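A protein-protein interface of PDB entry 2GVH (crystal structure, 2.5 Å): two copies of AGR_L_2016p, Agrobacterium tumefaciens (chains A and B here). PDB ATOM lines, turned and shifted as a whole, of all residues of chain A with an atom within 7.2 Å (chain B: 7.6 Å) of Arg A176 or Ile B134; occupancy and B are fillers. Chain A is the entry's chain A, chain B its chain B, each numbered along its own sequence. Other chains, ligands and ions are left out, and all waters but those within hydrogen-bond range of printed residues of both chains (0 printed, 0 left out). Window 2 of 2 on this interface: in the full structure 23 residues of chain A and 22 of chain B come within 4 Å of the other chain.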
ATOM      1  N   VAL A 166       8.012   2.008  -3.220  1.00  0.00           N
ATOM      2  CA  VAL A 166       8.212   1.632  -4.621  1.00  0.00           C
ATOM      3  C   VAL A 166       6.965   2.057  -5.387  1.00  0.00           C
ATOM      4  O   VAL A 166       5.862   1.602  -5.067  1.00  0.00           O
ATOM      5  CB  VAL A 166       8.392   0.120  -4.752  1.00  0.00           C
ATOM      6  CG1 VAL A 166       8.449  -0.300  -6.206  1.00  0.00           C
ATOM      7  CG2 VAL A 166       9.659  -0.315  -4.045  1.00  0.00           C
ATOM      8  N   PRO A 168       4.563   2.681  -8.899  1.00  0.00           N
ATOM      9  CA  PRO A 168       4.266   1.966 -10.163  1.00  0.00           C
ATOM     10  C   PRO A 168       5.247   2.283 -11.292  1.00  0.00           C
ATOM     11  O   PRO A 168       5.702   1.369 -11.989  1.00  0.00           O
ATOM     12  CB  PRO A 168       2.851   2.441 -10.521  1.00  0.00           C
ATOM     13  CG  PRO A 168       2.247   2.893  -9.195  1.00  0.00           C
ATOM     14  CD  PRO A 168       3.367   3.304  -8.292  1.00  0.00           C
ATOM     15  N   GLN A 170       8.244   2.833 -11.221  1.00  0.00           N
ATOM     16  CA  GLN A 170       9.530   2.178 -11.020  1.00  0.00           C
ATOM     17  C   GLN A 170       9.460   0.683 -11.203  1.00  0.00           C
ATOM     18  O   GLN A 170      10.463  -0.010 -11.035  1.00  0.00           O
ATOM     19  CB  GLN A 170      10.056   2.472  -9.648  1.00  0.00           C
ATOM     20  CG  GLN A 170      10.193   3.930  -9.358  1.00  0.00           C
ATOM     21  CD  GLN A 170      10.544   4.164  -7.908  1.00  0.00           C
ATOM     22  OE1 GLN A 170       9.700   4.070  -7.006  1.00  0.00           O
ATOM     23  NE2 GLN A 170      11.802   4.455  -7.670  1.00  0.00           N
ATOM     24  N   ALA A 171       8.283   0.179 -11.540  1.00  0.00           N
ATOM     25  CA  ALA A 171       8.077  -1.275 -11.613  1.00  0.00           C
ATOM     26  C   ALA A 171       7.649  -1.690 -12.993  1.00  0.00           C
ATOM     27  O   ALA A 171       7.035  -0.921 -13.711  1.00  0.00           O
ATOM     28  CB  ALA A 171       7.033  -1.714 -10.621  1.00  0.00           C
ATOM     29  N   ASN A 172       7.945  -2.925 -13.347  1.00  0.00           N
ATOM     30  CA  ASN A 172       7.525  -3.461 -14.616  1.00  0.00           C
ATOM     31  C   ASN A 172       6.152  -4.109 -14.507  1.00  0.00           C
ATOM     32  O   ASN A 172       5.577  -4.192 -13.411  1.00  0.00           O
ATOM     33  CB  ASN A 172       8.577  -4.447 -15.126  1.00  0.00           C
ATOM     34  CG  ASN A 172       8.681  -5.686 -14.269  1.00  0.00           C
ATOM     35  OD1 ASN A 172       7.674  -6.197 -13.756  1.00  0.00           O
ATOM     36  ND2 ASN A 172       9.904  -6.219 -14.150  1.00  0.00           N
ATOM     37  N   SER A 173       5.633  -4.586 -15.639  1.00  0.00           N
ATOM     38  CA  SER A 173       4.290  -5.162 -15.702  1.00  0.00           C
ATOM     39  C   SER A 173       4.173  -6.477 -14.927  1.00  0.00           C
ATOM     40  O   SER A 173       3.071  -6.987 -14.734  1.00  0.00           O
ATOM     41  CB  SER A 173       3.878  -5.391 -17.156  1.00  0.00           C
ATOM     42  OG  SER A 173       4.396  -6.630 -17.611  1.00  0.00           O
ATOM     43  N   ALA A 174       5.297  -7.046 -14.502  1.00  0.00           N
ATOM     44  CA  ALA A 174       5.234  -8.224 -13.635  1.00  0.00           C
ATOM     45  C   ALA A 174       5.135  -7.794 -12.161  1.00  0.00           C
ATOM     46  O   ALA A 174       5.065  -8.645 -11.269  1.00  0.00           O
ATOM     47  CB  ALA A 174       6.436  -9.130 -13.860  1.00  0.00           C
ATOM     48  N   GLY A 175       5.135  -6.478 -11.912  1.00  0.00           N
ATOM     49  CA  GLY A 175       5.038  -5.955 -10.553  1.00  0.00           C
ATOM     50  C   GLY A 175       6.372  -5.819  -9.855  1.00  0.00           C
ATOM     51  O   GLY A 175       6.427  -5.609  -8.647  1.00  0.00           O
ATOM     52  N   ARG A 176       7.460  -5.925 -10.610  1.00  0.00           N
ATOM     53  CA  ARG A 176       8.811  -5.917 -10.016  1.00  0.00           C
ATOM     54  C   ARG A 176       9.536  -4.606 -10.268  1.00  0.00           C
ATOM     55  O   ARG A 176       9.573  -4.110 -11.398  1.00  0.00           O
ATOM     56  CB  ARG A 176       9.647  -7.064 -10.562  1.00  0.00           C
ATOM     57  CG  ARG A 176       9.121  -8.442 -10.195  1.00  0.00           C
ATOM     58  CD  ARG A 176      10.078  -9.494 -10.697  1.00  0.00           C
ATOM     59  NE  ARG A 176       9.510 -10.839 -10.730  1.00  0.00           N
ATOM     60  CZ  ARG A 176       9.121 -11.459 -11.846  1.00  0.00           C
ATOM     61  NH1 ARG A 176       9.226 -10.833 -13.015  1.00  0.00           N
ATOM     62  NH2 ARG A 176       8.638 -12.705 -11.804  1.00  0.00           N
ATOM     63  N   MET A 177      10.111  -4.043  -9.215  1.00  0.00           N
ATOM     64  CA  MET A 177      10.917  -2.853  -9.355  1.00  0.00           C
ATOM     65  C   MET A 177      12.065  -3.158 -10.312  1.00  0.00           C
ATOM     66  O   MET A 177      12.693  -4.200 -10.208  1.00  0.00           O
ATOM     67  CB  MET A 177      11.453  -2.437  -7.996  1.00  0.00           C
ATOM     68  CG  MET A 177      12.238  -1.155  -8.018  1.00  0.00           C
ATOM     69  SD  MET A 177      12.954  -0.629  -6.217  1.00  0.00           S
ATOM     70  CE  MET A 177      12.965   1.319  -6.477  1.00  0.00           C
ATOM     71  N   PHE A 178      12.328  -2.255 -11.250  1.00  0.00           N
ATOM     72  CA  PHE A 178      13.536  -2.361 -12.081  1.00  0.00           C
ATOM     73  C   PHE A 178      14.746  -2.286 -11.175  1.00  0.00           C
ATOM     74  O   PHE A 178      14.792  -1.422 -10.277  1.00  0.00           O
ATOM     75  CB  PHE A 178      13.598  -1.232 -13.118  1.00  0.00           C
ATOM     76  CG  PHE A 178      12.505  -1.296 -14.122  1.00  0.00           C
ATOM     77  CD1 PHE A 178      12.518  -2.261 -15.136  1.00  0.00           C
ATOM     78  CD2 PHE A 178      11.438  -0.401 -14.051  1.00  0.00           C
ATOM     79  CE1 PHE A 178      11.469  -2.342 -16.090  1.00  0.00           C
ATOM     80  CE2 PHE A 178      10.367  -0.478 -14.996  1.00  0.00           C
ATOM     81  CZ  PHE A 178      10.396  -1.451 -16.025  1.00  0.00           C
ATOM     82  N   GLY A 179      15.701  -3.197 -11.389  1.00  0.00           N
ATOM     83  CA  GLY A 179      16.935  -3.173 -10.620  1.00  0.00           C
ATOM     84  C   GLY A 179      17.665  -1.850 -10.767  1.00  0.00           C
ATOM     85  O   GLY A 179      18.348  -1.379  -9.852  1.00  0.00           O
ATOM     86  N   ALA A 215      14.058  -9.974  -6.171  1.00  0.00           N
ATOM     87  CA  ALA A 215      13.417  -8.812  -6.791  1.00  0.00           C
ATOM     88  C   ALA A 215      12.467  -8.161  -5.807  1.00  0.00           C
ATOM     89  O   ALA A 215      11.801  -8.833  -5.029  1.00  0.00           O
ATOM     90  CB  ALA A 215      12.681  -9.201  -8.072  1.00  0.00           C
ATOM     91  N   ILE A 216      12.412  -6.841  -5.870  1.00  0.00           N
ATOM     92  CA  ILE A 216      11.610  -6.037  -4.991  1.00  0.00           C
ATOM     93  C   ILE A 216      10.267  -5.853  -5.640  1.00  0.00           C
ATOM     94  O   ILE A 216      10.199  -5.649  -6.855  1.00  0.00           O
ATOM     95  CB  ILE A 216      12.283  -4.672  -4.816  1.00  0.00           C
ATOM     96  CG1 ILE A 216      13.609  -4.870  -4.095  1.00  0.00           C
ATOM     97  CG2 ILE A 216      11.369  -3.689  -4.083  1.00  0.00           C
ATOM     98  CD1 ILE A 216      14.557  -3.725  -4.206  1.00  0.00           C
ATOM     99  N   GLU A 217       9.203  -5.918  -4.843  1.00  0.00           N
ATOM    100  CA  GLU A 217       7.846  -5.846  -5.381  1.00  0.00           C
ATOM    101  C   GLU A 217       7.122  -4.550  -5.076  1.00  0.00           C
ATOM    102  O   GLU A 217       7.458  -3.849  -4.121  1.00  0.00           O
ATOM    103  CB  GLU A 217       7.027  -7.058  -4.952  1.00  0.00           C
ATOM    104  CG  GLU A 217       7.175  -8.212  -5.927  1.00  0.00           C
ATOM    105  CD  GLU A 217       7.022  -9.570  -5.273  1.00  0.00           C
ATOM    106  OE1 GLU A 217       6.049  -9.763  -4.501  1.00  0.00           O
ATOM    107  OE2 GLU A 217       7.874 -10.451  -5.546  1.00  0.00           O
ATOM    108  N   ILE A 218       6.124  -4.252  -5.908  1.00  0.00           N
ATOM    109  CA  ILE A 218       5.362  -2.994  -5.873  1.00  0.00           C
ATOM    110  C   ILE A 218       4.773  -2.593  -4.493  1.00  0.00           C
ATOM    111  O   ILE A 218       4.824  -1.413  -4.110  1.00  0.00           O
ATOM    112  CB  ILE A 218       4.261  -2.993  -6.986  1.00  0.00           C
ATOM    113  CG1 ILE A 218       3.622  -1.608  -7.154  1.00  0.00           C
ATOM    114  CG2 ILE A 218       3.204  -4.088  -6.728  1.00  0.00           C
ATOM    115  CD1 ILE A 218       4.593  -0.528  -7.534  1.00  0.00           C
ATOM    116  N   PHE B  60      17.121  -4.028 -19.868  1.00  0.00           N
ATOM    117  CA  PHE B  60      15.884  -4.740 -19.670  1.00  0.00           C
ATOM    118  C   PHE B  60      15.110  -4.938 -20.981  1.00  0.00           C
ATOM    119  O   PHE B  60      14.831  -6.103 -21.394  1.00  0.00           O
ATOM    120  CB  PHE B  60      15.037  -4.033 -18.612  1.00  0.00           C
ATOM    121  CG  PHE B  60      13.637  -4.544 -18.517  1.00  0.00           C
ATOM    122  CD1 PHE B  60      13.348  -5.684 -17.791  1.00  0.00           C
ATOM    123  CD2 PHE B  60      12.602  -3.887 -19.154  1.00  0.00           C
ATOM    124  CE1 PHE B  60      12.050  -6.166 -17.698  1.00  0.00           C
ATOM    125  CE2 PHE B  60      11.294  -4.368 -19.071  1.00  0.00           C
ATOM    126  CZ  PHE B  60      11.020  -5.498 -18.334  1.00  0.00           C
ATOM    127  N   THR B  69      10.142 -12.825 -22.718  1.00  0.00           N
ATOM    128  CA  THR B  69       9.769 -13.442 -21.440  1.00  0.00           C
ATOM    129  C   THR B  69      10.126 -12.445 -20.354  1.00  0.00           C
ATOM    130  O   THR B  69      10.896 -11.552 -20.622  1.00  0.00           O
ATOM    131  CB  THR B  69      10.518 -14.790 -21.227  1.00  0.00           C
ATOM    132  OG1 THR B  69       9.956 -15.493 -20.113  1.00  0.00           O
ATOM    133  CG2 THR B  69      12.014 -14.573 -21.006  1.00  0.00           C
ATOM    134  N   PRO B  70       9.555 -12.557 -19.136  1.00  0.00           N
ATOM    135  CA  PRO B  70       9.980 -11.566 -18.129  1.00  0.00           C
ATOM    136  C   PRO B  70      11.450 -11.747 -17.719  1.00  0.00           C
ATOM    137  O   PRO B  70      11.949 -12.873 -17.691  1.00  0.00           O
ATOM    138  CB  PRO B  70       9.052 -11.835 -16.938  1.00  0.00           C
ATOM    139  CG  PRO B  70       7.926 -12.668 -17.496  1.00  0.00           C
ATOM    140  CD  PRO B  70       8.532 -13.473 -18.601  1.00  0.00           C
ATOM    141  N   PHE B  71      12.127 -10.636 -17.443  1.00  0.00           N
ATOM    142  CA  PHE B  71      13.510 -10.616 -16.978  1.00  0.00           C
ATOM    143  C   PHE B  71      13.690  -9.808 -15.706  1.00  0.00           C
ATOM    144  O   PHE B  71      13.010  -8.810 -15.491  1.00  0.00           O
ATOM    145  CB  PHE B  71      14.404  -9.962 -18.024  1.00  0.00           C
ATOM    146  CG  PHE B  71      14.816 -10.873 -19.114  1.00  0.00           C
ATOM    147  CD1 PHE B  71      15.909 -11.677 -18.970  1.00  0.00           C
ATOM    148  CD2 PHE B  71      14.090 -10.939 -20.286  1.00  0.00           C
ATOM    149  CE1 PHE B  71      16.281 -12.526 -19.969  1.00  0.00           C
ATOM    150  CE2 PHE B  71      14.450 -11.787 -21.285  1.00  0.00           C
ATOM    151  CZ  PHE B  71      15.553 -12.575 -21.136  1.00  0.00           C
ATOM    152  N   VAL B  72      14.647 -10.219 -14.891  1.00  0.00           N
ATOM    153  CA  VAL B  72      15.116  -9.385 -13.797  1.00  0.00           C
ATOM    154  C   VAL B  72      16.612  -9.154 -13.935  1.00  0.00           C
ATOM    155  O   VAL B  72      17.311  -9.854 -14.691  1.00  0.00           O
ATOM    156  CB  VAL B  72      14.852 -10.014 -12.428  1.00  0.00           C
ATOM    157  CG1 VAL B  72      13.363 -10.071 -12.168  1.00  0.00           C
ATOM    158  CG2 VAL B  72      15.529 -11.424 -12.304  1.00  0.00           C
ATOM    159  N   THR B  73      17.103  -8.180 -13.188  1.00  0.00           N
ATOM    160  CA  THR B  73      18.505  -7.880 -13.165  1.00  0.00           C
ATOM    161  C   THR B  73      19.132  -8.632 -12.015  1.00  0.00           C
ATOM    162  O   THR B  73      18.886  -8.319 -10.850  1.00  0.00           O
ATOM    163  CB  THR B  73      18.710  -6.418 -13.037  1.00  0.00           C
ATOM    164  OG1 THR B  73      18.085  -5.794 -14.150  1.00  0.00           O
ATOM    165  CG2 THR B  73      20.170  -6.087 -13.071  1.00  0.00           C
ATOM    166  N   ARG B 103      19.264 -19.338 -19.296  1.00  0.00           N
ATOM    167  CA  ARG B 103      18.435 -18.307 -18.669  1.00  0.00           C
ATOM    168  C   ARG B 103      19.136 -16.974 -18.351  1.00  0.00           C
ATOM    169  O   ARG B 103      18.483 -15.957 -18.043  1.00  0.00           O
ATOM    170  CB  ARG B 103      17.705 -18.862 -17.448  1.00  0.00           C
ATOM    171  CG  ARG B 103      16.328 -19.387 -17.817  1.00  0.00           C
ATOM    172  CD  ARG B 103      15.756 -20.297 -16.755  1.00  0.00           C
ATOM    173  NE  ARG B 103      14.822 -21.281 -17.314  1.00  0.00           N
ATOM    174  CZ  ARG B 103      13.705 -21.661 -16.704  1.00  0.00           C
ATOM    175  NH1 ARG B 103      13.378 -21.155 -15.524  1.00  0.00           N
ATOM    176  NH2 ARG B 103      12.908 -22.538 -17.277  1.00  0.00           N
ATOM    177  N   MET B 131      21.099 -10.131 -17.043  1.00  0.00           N
ATOM    178  CA  MET B 131      19.662 -10.353 -16.891  1.00  0.00           C
ATOM    179  C   MET B 131      19.440 -11.844 -16.759  1.00  0.00           C
ATOM    180  O   MET B 131      20.255 -12.618 -17.208  1.00  0.00           O
ATOM    181  CB  MET B 131      18.881  -9.818 -18.078  1.00  0.00           C
ATOM    182  CG  MET B 131      19.288  -8.429 -18.535  1.00  0.00           C
ATOM    183  SD  MET B 131      19.286  -7.121 -17.110  1.00  0.00           S
ATOM    184  CE  MET B 131      17.355  -6.851 -16.872  1.00  0.00           C
ATOM    185  N   VAL B 132      18.356 -12.222 -16.091  1.00  0.00           N
ATOM    186  CA  VAL B 132      17.936 -13.599 -15.932  1.00  0.00           C
ATOM    187  C   VAL B 132      16.452 -13.648 -16.255  1.00  0.00           C
ATOM    188  O   VAL B 132      15.690 -12.742 -15.886  1.00  0.00           O
ATOM    189  CB  VAL B 132      18.162 -14.089 -14.496  1.00  0.00           C
ATOM    190  CG1 VAL B 132      17.528 -15.461 -14.271  1.00  0.00           C
ATOM    191  CG2 VAL B 132      19.632 -14.133 -14.173  1.00  0.00           C
ATOM    192  N   ALA B 133      16.061 -14.703 -16.969  1.00  0.00           N
ATOM    193  CA  ALA B 133      14.687 -14.875 -17.410  1.00  0.00           C
ATOM    194  C   ALA B 133      13.901 -15.519 -16.296  1.00  0.00           C
ATOM    195  O   ALA B 133      14.365 -16.485 -15.707  1.00  0.00           O
ATOM    196  CB  ALA B 133      14.659 -15.763 -18.642  1.00  0.00           C
ATOM    197  N   ILE B 134      12.723 -14.988 -15.992  1.00  0.00           N
ATOM    198  CA  ILE B 134      11.788 -15.680 -15.091  1.00  0.00           C
ATOM    199  C   ILE B 134      10.523 -15.979 -15.879  1.00  0.00           C
ATOM    200  O   ILE B 134       9.570 -15.202 -15.850  1.00  0.00           O
ATOM    201  CB  ILE B 134      11.414 -14.842 -13.838  1.00  0.00           C
ATOM    202  CG1 ILE B 134      12.661 -14.238 -13.161  1.00  0.00           C
ATOM    203  CG2 ILE B 134      10.559 -15.683 -12.883  1.00  0.00           C
ATOM    204  CD1 ILE B 134      13.475 -15.189 -12.357  1.00  0.00           C
ATOM    205  N   PRO B 135      10.517 -17.102 -16.597  1.00  0.00           N
ATOM    206  CA  PRO B 135       9.377 -17.417 -17.453  1.00  0.00           C
ATOM    207  C   PRO B 135       8.134 -17.805 -16.655  1.00  0.00           C
ATOM    208  O   PRO B 135       8.239 -18.433 -15.594  1.00  0.00           O
ATOM    209  CB  PRO B 135       9.884 -18.601 -18.283  1.00  0.00           C
ATOM    210  CG  PRO B 135      10.911 -19.259 -17.410  1.00  0.00           C
ATOM    211  CD  PRO B 135      11.564 -18.140 -16.645  1.00  0.00           C
ATOM    212  N   GLU B 136       6.972 -17.412 -17.177  1.00  0.00           N
ATOM    213  CA  GLU B 136       5.670 -17.765 -16.612  1.00  0.00           C
ATOM    214  C   GLU B 136       4.938 -18.725 -17.570  1.00  0.00           C
ATOM    215  O   GLU B 136       5.349 -18.885 -18.725  1.00  0.00           O
ATOM    216  CB  GLU B 136       4.855 -16.484 -16.370  1.00  0.00           C
ATOM    217  N   GLY B 137       3.874 -19.371 -17.101  1.00  0.00           N
ATOM    218  CA  GLY B 137       3.078 -20.238 -17.970  1.00  0.00           C
ATOM    219  C   GLY B 137       3.198 -21.715 -17.680  1.00  0.00           C
ATOM    220  O   GLY B 137       3.954 -22.125 -16.797  1.00  0.00           O
ATOM    221  N   ALA B 140       6.678 -23.251 -18.695  1.00  0.00           N
ATOM    222  CA  ALA B 140       7.798 -22.457 -18.173  1.00  0.00           C
ATOM    223  C   ALA B 140       8.935 -23.314 -17.600  1.00  0.00           C
ATOM    224  O   ALA B 140      10.099 -22.920 -17.644  1.00  0.00           O
ATOM    225  CB  ALA B 140       7.310 -21.440 -17.138  1.00  0.00           C
ATOM    226  N   TYR B 143      11.444 -23.410 -20.444  1.00  0.00           N
ATOM    227  CA  TYR B 143      11.849 -22.240 -21.214  1.00  0.00           C
ATOM    228  C   TYR B 143      13.359 -22.237 -21.367  1.00  0.00           C
ATOM    229  O   TYR B 143      14.083 -22.446 -20.390  1.00  0.00           O
ATOM    230  CB  TYR B 143      11.440 -20.941 -20.520  1.00  0.00           C
ATOM    231  CG  TYR B 143      12.045 -19.757 -21.242  1.00  0.00           C
ATOM    232  CD1 TYR B 143      11.415 -19.219 -22.356  1.00  0.00           C
ATOM    233  CD2 TYR B 143      13.288 -19.246 -20.877  1.00  0.00           C
ATOM    234  CE1 TYR B 143      11.971 -18.182 -23.064  1.00  0.00           C
ATOM    235  CE2 TYR B 143      13.859 -18.198 -21.586  1.00  0.00           C
ATOM    236  CZ  TYR B 143      13.187 -17.669 -22.678  1.00  0.00           C
ATOM    237  OH  TYR B 143      13.722 -16.651 -23.416  1.00  0.00           O
ATOM    238  N   LEU B 248       6.356  -9.008 -24.691  1.00  0.00           N
ATOM    239  CA  LEU B 248       6.419 -10.442 -24.509  1.00  0.00           C
ATOM    240  C   LEU B 248       6.132 -11.203 -25.795  1.00  0.00           C
ATOM    241  O   LEU B 248       6.718 -12.243 -26.034  1.00  0.00           O
ATOM    242  CB  LEU B 248       5.483 -10.882 -23.381  1.00  0.00           C
ATOM    243  CG  LEU B 248       5.777 -10.276 -22.001  1.00  0.00           C
ATOM    244  CD1 LEU B 248       4.641 -10.531 -20.989  1.00  0.00           C
ATOM    245  CD2 LEU B 248       7.112 -10.766 -21.466  1.00  0.00           C
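Hydrophobic or aromatic side chains of chain A that line the printed part of chain B: Phe A178.
Of the 17 printed residues of chain B, 3 touch a printed residue of chain A.
Printed residues of chain B that touch a printed residue of chain A: Phe B60, Val B72 and Ile B134.
Hydrophobic or aromatic side chains of chain B that line the printed part of chain A: Phe B60, Val B72 and Ile B134.
Among the printed residues, 3 pairs touch across the chains.
No position is printed for both chains.
Of the 3 pairs that touch across the chains among the printed residues, none has its exchanged pair printed and touching as well.
Arg A176 touches just these residues of chain B: Val B72 (3.6 Å) and Ile B134 (3.7 Å).
Ile B134 touches just one residue of chain A: Arg A176.
Of the printed residues of chain A, Val B72 touches Arg A176.
Of the printed residues of chain B, Phe A178 touches Phe B60 (3.6 Å).
Of the printed residues of chain A, Phe B60 touches Phe A178.
Leu B248 touches none of the printed residues of chain A.
The nearest residue of chain B that does not touch Arg A176 is Pro B70 (4.1 Å).
The nearest residue of chain A that does not touch Ile B134 is Ala A174 (7.1 Å).
Val B72 touches Arg A176.
Arg A176 touches Ile B134.
CE1 of Phe A178 touches CE2 of Phe B60, at 3.6 Å.
N of Arg A176 sits at hydrogen-bond distance from OD1 of Asn A172, 3.2 Å away.
The backbone carbonyl oxygen (O) of Gln A170 sits at hydrogen-bond distance from the backbone NH (N) of Phe A178, 2.9 Å away.
The backbone carbonyl oxygen (O) of Pro B70 lies within hydrogen-bond range of the backbone NH (N) of Ile B134, 2.8 Å away.
The backbone NH of Val B72 is in hydrogen-bond range of the backbone carbonyl oxygen of Val B132, at 2.9 Å.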
